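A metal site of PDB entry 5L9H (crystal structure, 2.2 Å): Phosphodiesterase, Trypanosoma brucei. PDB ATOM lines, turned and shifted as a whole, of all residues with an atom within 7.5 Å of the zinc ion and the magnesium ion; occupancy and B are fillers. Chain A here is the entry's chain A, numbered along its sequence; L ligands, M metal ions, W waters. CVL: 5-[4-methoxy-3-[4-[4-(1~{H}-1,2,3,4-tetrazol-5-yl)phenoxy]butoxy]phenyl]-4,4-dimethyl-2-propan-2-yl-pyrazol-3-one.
The backbone carbonyl oxygen (O) of Ala 148 lies within hydrogen-bond range of a ring nitrogen (ND1) of His 151 (2.6 Å).
The nearest printed residue that does not touch the magnesium ion is His 151 (4.1 Å).
The zinc ion is bound by water W3 (2.1 Å), OD1 of Asp 264 (2.2 Å), OD2 of Asp 152 (2.2 Å), NE2 of His 115 (2.2 Å) and NE2 of His 151 (2.4 Å). The zinc ion has five donor atoms within binding distance. Slightly farther from the zinc ion lies water W1 (2.8 Å).
The magnesium ion is bound by water W2 (2.0 Å), water W3 (2.1 Å), water W4 (2.1 Å), water W6 (2.1 Å), OD1 of Asp 152 (2.1 Å) and water W5 (2.3 Å). The magnesium ion has six donor atoms within binding distance.
Of the 21 residues printed, 4 come within 4 Å of the zinc ion. The nearest printed residue that does not touch the zinc ion is His 111 (4.1 Å).
Water W1 lies within hydrogen-bond range of a ring nitrogen (NE2) of His 111 (2.8 Å) and the side-chain carboxylate (OD2) of Asp 264 (3.5 Å). Water W6 lies within hydrogen-bond range of the backbone carbonyl oxygen of His 151 (2.6 Å) and the side-chain hydroxyl of Thr 225 (2.8 Å). Water W2 lies within hydrogen-bond range of NE2 of His 187 and OE2 of Glu 184. Water W5 lies within hydrogen-bond range of O of Thr 225 (2.9 Å) and OE2 of Glu 184 (3.0 Å).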
ATOM      1  N   TYR A 110      -3.636  -4.930 -16.103  1.00  0.00           N
ATOM      2  CA  TYR A 110      -2.600  -4.931 -17.168  1.00  0.00           C
ATOM      3  C   TYR A 110      -2.427  -3.560 -17.890  1.00  0.00           C
ATOM      4  O   TYR A 110      -1.365  -2.975 -17.836  1.00  0.00           O
ATOM      5  CB  TYR A 110      -2.920  -6.004 -18.192  1.00  0.00           C
ATOM      6  CG  TYR A 110      -1.887  -6.153 -19.293  1.00  0.00           C
ATOM      7  CD1 TYR A 110      -0.677  -6.794 -19.055  1.00  0.00           C
ATOM      8  CD2 TYR A 110      -2.120  -5.669 -20.571  1.00  0.00           C
ATOM      9  CE1 TYR A 110       0.272  -6.953 -20.059  1.00  0.00           C
ATOM     10  CE2 TYR A 110      -1.168  -5.810 -21.588  1.00  0.00           C
ATOM     11  CZ  TYR A 110       0.026  -6.455 -21.322  1.00  0.00           C
ATOM     12  OH  TYR A 110       0.960  -6.611 -22.309  1.00  0.00           O
ATOM     13  N   HIS A 111      -3.487  -3.044 -18.518  1.00  0.00           N
ATOM     14  CA  HIS A 111      -3.408  -1.808 -19.288  1.00  0.00           C
ATOM     15  C   HIS A 111      -3.392  -0.505 -18.491  1.00  0.00           C
ATOM     16  O   HIS A 111      -4.232   0.360 -18.674  1.00  0.00           O
ATOM     17  CB  HIS A 111      -4.492  -1.777 -20.324  1.00  0.00           C
ATOM     18  CG  HIS A 111      -4.332  -2.809 -21.380  1.00  0.00           C
ATOM     19  ND1 HIS A 111      -5.157  -3.899 -21.464  1.00  0.00           N
ATOM     20  CD2 HIS A 111      -3.478  -2.918 -22.415  1.00  0.00           C
ATOM     21  CE1 HIS A 111      -4.862  -4.597 -22.551  1.00  0.00           C
ATOM     22  NE2 HIS A 111      -3.827  -4.029 -23.137  1.00  0.00           N
ATOM     23  N   HIS A 115       2.212  -0.784 -17.792  1.00  0.00           N
ATOM     24  CA  HIS A 115       2.289  -1.342 -19.131  1.00  0.00           C
ATOM     25  C   HIS A 115       2.971  -0.406 -20.167  1.00  0.00           C
ATOM     26  O   HIS A 115       3.780  -0.851 -20.984  1.00  0.00           O
ATOM     27  CB  HIS A 115       0.908  -1.771 -19.619  1.00  0.00           C
ATOM     28  CG  HIS A 115       0.873  -2.090 -21.080  1.00  0.00           C
ATOM     29  ND1 HIS A 115       1.584  -3.125 -21.635  1.00  0.00           N
ATOM     30  CD2 HIS A 115       0.215  -1.491 -22.111  1.00  0.00           C
ATOM     31  CE1 HIS A 115       1.351  -3.183 -22.938  1.00  0.00           C
ATOM     32  NE2 HIS A 115       0.553  -2.180 -23.252  1.00  0.00           N
ATOM     33  N   VAL A 116       2.651   0.875 -20.141  1.00  0.00           N
ATOM     34  CA  VAL A 116       3.156   1.742 -21.215  1.00  0.00           C
ATOM     35  C   VAL A 116       4.556   2.194 -20.945  1.00  0.00           C
ATOM     36  O   VAL A 116       5.280   2.433 -21.886  1.00  0.00           O
ATOM     37  CB  VAL A 116       2.224   2.939 -21.563  1.00  0.00           C
ATOM     38  CG1 VAL A 116       0.835   2.437 -21.884  1.00  0.00           C
ATOM     39  CG2 VAL A 116       2.146   4.004 -20.463  1.00  0.00           C
ATOM     40  N   VAL A 119       6.434  -0.661 -22.287  1.00  0.00           N
ATOM     41  CA  VAL A 119       6.540  -0.603 -23.763  1.00  0.00           C
ATOM     42  C   VAL A 119       7.560   0.425 -24.217  1.00  0.00           C
ATOM     43  O   VAL A 119       8.336   0.136 -25.143  1.00  0.00           O
ATOM     44  CB  VAL A 119       5.194  -0.340 -24.411  1.00  0.00           C
ATOM     45  CG1 VAL A 119       5.318  -0.075 -25.911  1.00  0.00           C
ATOM     46  CG2 VAL A 119       4.285  -1.554 -24.179  1.00  0.00           C
ATOM     47  N   ALA A 148       4.869   5.348 -27.243  1.00  0.00           N
ATOM     48  CA  ALA A 148       4.739   4.296 -26.247  1.00  0.00           C
ATOM     49  C   ALA A 148       3.893   4.726 -25.050  1.00  0.00           C
ATOM     50  O   ALA A 148       3.052   3.982 -24.607  1.00  0.00           O
ATOM     51  CB  ALA A 148       6.080   3.853 -25.765  1.00  0.00           C
ATOM     52  N   HIS A 151      -0.136   5.256 -25.892  1.00  0.00           N
ATOM     53  CA  HIS A 151      -0.825   4.343 -26.863  1.00  0.00           C
ATOM     54  C   HIS A 151      -1.974   3.547 -26.283  1.00  0.00           C
ATOM     55  O   HIS A 151      -2.662   2.835 -27.029  1.00  0.00           O
ATOM     56  CB  HIS A 151       0.174   3.401 -27.504  1.00  0.00           C
ATOM     57  CG  HIS A 151       0.481   2.196 -26.672  1.00  0.00           C
ATOM     58  ND1 HIS A 151       1.382   2.225 -25.638  1.00  0.00           N
ATOM     59  CD2 HIS A 151      -0.003   0.932 -26.730  1.00  0.00           C
ATOM     60  CE1 HIS A 151       1.444   1.027 -25.082  1.00  0.00           C
ATOM     61  NE2 HIS A 151       0.587   0.241 -25.718  1.00  0.00           N
ATOM     62  N   ASP A 152      -2.128   3.630 -24.947  1.00  0.00           N
ATOM     63  CA  ASP A 152      -3.261   3.015 -24.251  1.00  0.00           C
ATOM     64  C   ASP A 152      -4.022   3.976 -23.308  1.00  0.00           C
ATOM     65  O   ASP A 152      -4.744   3.513 -22.430  1.00  0.00           O
ATOM     66  CB  ASP A 152      -2.758   1.781 -23.473  1.00  0.00           C
ATOM     67  CG  ASP A 152      -2.715   0.534 -24.340  1.00  0.00           C
ATOM     68  OD1 ASP A 152      -3.536   0.394 -25.284  1.00  0.00           O
ATOM     69  OD2 ASP A 152      -1.851  -0.319 -24.080  1.00  0.00           O
ATOM     70  N   LEU A 153      -3.887   5.285 -23.516  1.00  0.00           N
ATOM     71  CA  LEU A 153      -4.490   6.269 -22.635  1.00  0.00           C
ATOM     72  C   LEU A 153      -5.959   5.969 -22.334  1.00  0.00           C
ATOM     73  O   LEU A 153      -6.728   5.773 -23.235  1.00  0.00           O
ATOM     74  CB  LEU A 153      -4.393   7.670 -23.203  1.00  0.00           C
ATOM     75  CG  LEU A 153      -3.029   8.331 -23.209  1.00  0.00           C
ATOM     76  CD1 LEU A 153      -3.088   9.567 -24.135  1.00  0.00           C
ATOM     77  CD2 LEU A 153      -2.555   8.737 -21.820  1.00  0.00           C
ATOM     78  N   HIS A 155      -7.421   3.349 -20.982  1.00  0.00           N
ATOM     79  CA  HIS A 155      -7.886   1.944 -21.082  1.00  0.00           C
ATOM     80  C   HIS A 155      -8.619   1.581 -19.798  1.00  0.00           C
ATOM     81  O   HIS A 155      -8.142   1.929 -18.689  1.00  0.00           O
ATOM     82  CB  HIS A 155      -6.675   0.977 -21.264  1.00  0.00           C
ATOM     83  CG  HIS A 155      -6.947  -0.195 -22.144  1.00  0.00           C
ATOM     84  ND1 HIS A 155      -7.672  -1.275 -21.727  1.00  0.00           N
ATOM     85  CD2 HIS A 155      -6.600  -0.444 -23.436  1.00  0.00           C
ATOM     86  CE1 HIS A 155      -7.782  -2.150 -22.718  1.00  0.00           C
ATOM     87  NE2 HIS A 155      -7.135  -1.671 -23.762  1.00  0.00           N
ATOM     88  N   LEU A 183     -11.052   1.641 -29.337  1.00  0.00           N
ATOM     89  CA  LEU A 183     -10.129   2.164 -28.377  1.00  0.00           C
ATOM     90  C   LEU A 183      -8.953   2.930 -28.894  1.00  0.00           C
ATOM     91  O   LEU A 183      -8.494   3.848 -28.258  1.00  0.00           O
ATOM     92  CB  LEU A 183      -9.597   1.021 -27.536  1.00  0.00           C
ATOM     93  CG  LEU A 183     -10.516   0.456 -26.477  1.00  0.00           C
ATOM     94  CD1 LEU A 183     -10.028  -0.885 -26.037  1.00  0.00           C
ATOM     95  CD2 LEU A 183     -10.583   1.383 -25.296  1.00  0.00           C
ATOM     96  N   GLU A 184      -8.459   2.527 -30.031  1.00  0.00           N
ATOM     97  CA  GLU A 184      -7.222   3.126 -30.555  1.00  0.00           C
ATOM     98  C   GLU A 184      -7.489   4.562 -30.972  1.00  0.00           C
ATOM     99  O   GLU A 184      -6.654   5.448 -30.765  1.00  0.00           O
ATOM    100  CB  GLU A 184      -6.630   2.282 -31.693  1.00  0.00           C
ATOM    101  CG  GLU A 184      -6.084   0.930 -31.238  1.00  0.00           C
ATOM    102  CD  GLU A 184      -7.140  -0.111 -30.810  1.00  0.00           C
ATOM    103  OE1 GLU A 184      -8.341   0.082 -31.110  1.00  0.00           O
ATOM    104  OE2 GLU A 184      -6.759  -1.116 -30.154  1.00  0.00           O
ATOM    105  N   HIS A 187      -7.580   6.504 -27.773  1.00  0.00           N
ATOM    106  CA  HIS A 187      -6.211   6.805 -27.327  1.00  0.00           C
ATOM    107  C   HIS A 187      -5.630   7.985 -28.097  1.00  0.00           C
ATOM    108  O   HIS A 187      -5.039   8.869 -27.498  1.00  0.00           O
ATOM    109  CB  HIS A 187      -5.254   5.606 -27.399  1.00  0.00           C
ATOM    110  CG  HIS A 187      -5.774   4.349 -26.768  1.00  0.00           C
ATOM    111  ND1 HIS A 187      -6.332   4.339 -25.508  1.00  0.00           N
ATOM    112  CD2 HIS A 187      -5.826   3.085 -27.227  1.00  0.00           C
ATOM    113  CE1 HIS A 187      -6.720   3.106 -25.226  1.00  0.00           C
ATOM    114  NE2 HIS A 187      -6.448   2.336 -26.263  1.00  0.00           N
ATOM    115  N   VAL A 222      -0.362   4.193 -33.315  1.00  0.00           N
ATOM    116  CA  VAL A 222      -1.347   3.792 -32.269  1.00  0.00           C
ATOM    117  C   VAL A 222      -2.490   3.030 -32.913  1.00  0.00           C
ATOM    118  O   VAL A 222      -2.900   2.012 -32.394  1.00  0.00           O
ATOM    119  CB  VAL A 222      -1.896   4.995 -31.520  1.00  0.00           C
ATOM    120  CG1 VAL A 222      -3.044   4.598 -30.617  1.00  0.00           C
ATOM    121  CG2 VAL A 222      -0.764   5.658 -30.746  1.00  0.00           C
ATOM    122  N   THR A 225      -1.777  -0.743 -33.437  1.00  0.00           N
ATOM    123  CA  THR A 225      -1.773  -1.646 -32.302  1.00  0.00           C
ATOM    124  C   THR A 225      -3.090  -2.416 -32.150  1.00  0.00           C
ATOM    125  O   THR A 225      -3.170  -3.326 -31.315  1.00  0.00           O
ATOM    126  CB  THR A 225      -1.506  -0.925 -30.976  1.00  0.00           C
ATOM    127  OG1 THR A 225      -2.537   0.043 -30.732  1.00  0.00           O
ATOM    128  CG2 THR A 225      -0.183  -0.189 -31.026  1.00  0.00           C
ATOM    129  N   ASP A 226      -4.129  -2.068 -32.921  1.00  0.00           N
ATOM    130  CA  ASP A 226      -5.360  -2.868 -32.921  1.00  0.00           C
ATOM    131  C   ASP A 226      -5.045  -4.301 -33.421  1.00  0.00           C
ATOM    132  O   ASP A 226      -4.712  -4.492 -34.561  1.00  0.00           O
ATOM    133  CB  ASP A 226      -6.434  -2.200 -33.789  1.00  0.00           C
ATOM    134  CG  ASP A 226      -7.753  -2.996 -33.852  1.00  0.00           C
ATOM    135  OD1 ASP A 226      -7.815  -4.198 -33.470  1.00  0.00           O
ATOM    136  OD2 ASP A 226      -8.727  -2.406 -34.318  1.00  0.00           O
ATOM    137  N   MET A 227      -5.209  -5.279 -32.540  1.00  0.00           N
ATOM    138  CA  MET A 227      -4.849  -6.679 -32.838  1.00  0.00           C
ATOM    139  C   MET A 227      -5.658  -7.335 -33.946  1.00  0.00           C
ATOM    140  O   MET A 227      -5.183  -8.293 -34.537  1.00  0.00           O
ATOM    141  CB  MET A 227      -4.861  -7.552 -31.587  1.00  0.00           C
ATOM    142  CG  MET A 227      -3.570  -7.451 -30.727  1.00  0.00           C
ATOM    143  SD  MET A 227      -1.945  -7.698 -31.508  1.00  0.00           S
ATOM    144  CE  MET A 227      -2.075  -9.376 -32.096  1.00  0.00           C
ATOM    145  N   LEU A 260       6.200  -0.531 -32.544  1.00  0.00           N
ATOM    146  CA  LEU A 260       5.233  -0.273 -31.500  1.00  0.00           C
ATOM    147  C   LEU A 260       4.461  -1.551 -31.246  1.00  0.00           C
ATOM    148  O   LEU A 260       4.213  -1.899 -30.145  1.00  0.00           O
ATOM    149  CB  LEU A 260       4.294   0.888 -31.823  1.00  0.00           C
ATOM    150  CG  LEU A 260       3.336   1.244 -30.680  1.00  0.00           C
ATOM    151  CD1 LEU A 260       4.044   1.606 -29.416  1.00  0.00           C
ATOM    152  CD2 LEU A 260       2.291   2.260 -30.990  1.00  0.00           C
ATOM    153  N   GLY A 263       6.727  -3.917 -29.315  1.00  0.00           N
ATOM    154  CA  GLY A 263       6.787  -3.549 -27.910  1.00  0.00           C
ATOM    155  C   GLY A 263       5.544  -3.999 -27.175  1.00  0.00           C
ATOM    156  O   GLY A 263       5.622  -4.396 -26.022  1.00  0.00           O
ATOM    157  N   ASP A 264       4.408  -3.976 -27.856  1.00  0.00           N
ATOM    158  CA  ASP A 264       3.143  -4.283 -27.235  1.00  0.00           C
ATOM    159  C   ASP A 264       2.945  -5.777 -26.945  1.00  0.00           C
ATOM    160  O   ASP A 264       2.329  -6.113 -25.941  1.00  0.00           O
ATOM    161  CB  ASP A 264       2.005  -3.782 -28.150  1.00  0.00           C
ATOM    162  CG  ASP A 264       0.849  -3.215 -27.382  1.00  0.00           C
ATOM    163  OD1 ASP A 264       1.001  -2.818 -26.201  1.00  0.00           O
ATOM    164  OD2 ASP A 264      -0.221  -3.163 -27.991  1.00  0.00           O
ATOM    165  N   ILE A 265       3.464  -6.643 -27.815  1.00  0.00           N
ATOM    166  CA  ILE A 265       3.481  -8.083 -27.559  1.00  0.00           C
ATOM    167  C   ILE A 265       4.854  -8.642 -27.090  1.00  0.00           C
ATOM    168  O   ILE A 265       5.178  -9.793 -27.306  1.00  0.00           O
ATOM    169  CB  ILE A 265       2.961  -8.852 -28.767  1.00  0.00           C
ATOM    170  CG1 ILE A 265       3.840  -8.700 -29.989  1.00  0.00           C
ATOM    171  CG2 ILE A 265       1.553  -8.388 -29.091  1.00  0.00           C
ATOM    172  CD1 ILE A 265       3.326  -9.519 -31.135  1.00  0.00           C
HETATM  173  C1  CVL L   1       1.721 -11.967 -21.209  1.00  0.00           C
HETATM  174  O1  CVL L   1       0.970 -12.713 -22.172  1.00  0.00           O
HETATM  175  C2  CVL L   1       0.163 -12.038 -23.043  1.00  0.00           C
HETATM  176  C3  CVL L   1       0.339 -10.739 -23.469  1.00  0.00           C
HETATM  177  C4  CVL L   1      -0.545 -10.167 -24.370  1.00  0.00           C
HETATM  178  C5  CVL L   1      -1.628 -10.898 -24.870  1.00  0.00           C
HETATM  179  C6  CVL L   1      -2.556 -10.316 -25.845  1.00  0.00           C
HETATM  180  N1  CVL L   1      -3.110 -11.078 -26.729  1.00  0.00           N
HETATM  181  N2  CVL L   1      -4.146 -10.366 -27.273  1.00  0.00           N
HETATM  182  C7  CVL L   1      -5.102 -11.107 -28.149  1.00  0.00           C
HETATM  183  C8  CVL L   1      -6.179 -10.196 -28.729  1.00  0.00           C
HETATM  184  C9  CVL L   1      -4.321 -11.836 -29.213  1.00  0.00           C
HETATM  185  C10 CVL L   1      -4.119  -9.049 -26.924  1.00  0.00           C
HETATM  186  O2  CVL L   1      -4.848  -8.147 -27.277  1.00  0.00           O
HETATM  187  C11 CVL L   1      -2.949  -8.866 -25.981  1.00  0.00           C
HETATM  188  C12 CVL L   1      -1.848  -8.033 -26.662  1.00  0.00           C
HETATM  189  C13 CVL L   1      -3.388  -8.213 -24.669  1.00  0.00           C
HETATM  190  C14 CVL L   1      -1.791 -12.221 -24.458  1.00  0.00           C
HETATM  191  C15 CVL L   1      -0.919 -12.791 -23.550  1.00  0.00           C
HETATM  192  O3  CVL L   1      -1.067 -14.079 -23.109  1.00  0.00           O
HETATM  193  C16 CVL L   1      -2.289 -14.444 -22.457  1.00  0.00           C
HETATM  194  C17 CVL L   1      -2.527 -15.916 -22.702  1.00  0.00           C
HETATM  195  C18 CVL L   1      -3.916 -16.318 -23.155  1.00  0.00           C
HETATM  196  C19 CVL L   1      -3.930 -17.153 -24.423  1.00  0.00           C
HETATM  197  O4  CVL L   1      -3.391 -16.334 -25.470  1.00  0.00           O
HETATM  198  C20 CVL L   1      -3.556 -16.710 -26.773  1.00  0.00           C
HETATM  199  C21 CVL L   1      -3.389 -18.012 -27.205  1.00  0.00           C
HETATM  200  C22 CVL L   1      -3.566 -18.333 -28.542  1.00  0.00           C
HETATM  201  C23 CVL L   1      -3.916 -17.355 -29.467  1.00  0.00           C
HETATM  202  C24 CVL L   1      -4.097 -17.688 -30.876  1.00  0.00           C
HETATM  203  N3  CVL L   1      -4.281 -18.903 -31.384  1.00  0.00           N
HETATM  204  N4  CVL L   1      -4.380 -18.752 -32.726  1.00  0.00           N
HETATM  205  N5  CVL L   1      -4.271 -17.501 -33.044  1.00  0.00           N
HETATM  206  N6  CVL L   1      -4.097 -16.827 -31.898  1.00  0.00           N
HETATM  207  C25 CVL L   1      -4.085 -16.052 -29.025  1.00  0.00           C
HETATM  208  C26 CVL L   1      -3.908 -15.731 -27.688  1.00  0.00           C
HETATM  209 ZN    ZN M   1      -0.570  -1.782 -25.124  1.00  0.00          ZN
HETATM  210 MG    MG M   2      -3.959  -1.033 -26.808  1.00  0.00          MG
HETATM  211  O   HOH W   1      -1.974  -4.226 -25.167  1.00  0.00           O
HETATM  212  O   HOH W   2      -5.949  -0.637 -26.930  1.00  0.00           O
HETATM  213  O   HOH W   3      -1.984  -1.651 -26.681  1.00  0.00           O
HETATM  214  O   HOH W   4      -4.707  -2.889 -26.245  1.00  0.00           O
HETATM  215  O   HOH W   5      -4.113  -1.959 -28.946  1.00  0.00           O
HETATM  216  O   HOH W   6      -3.450   0.571 -28.089  1.00  0.00           O
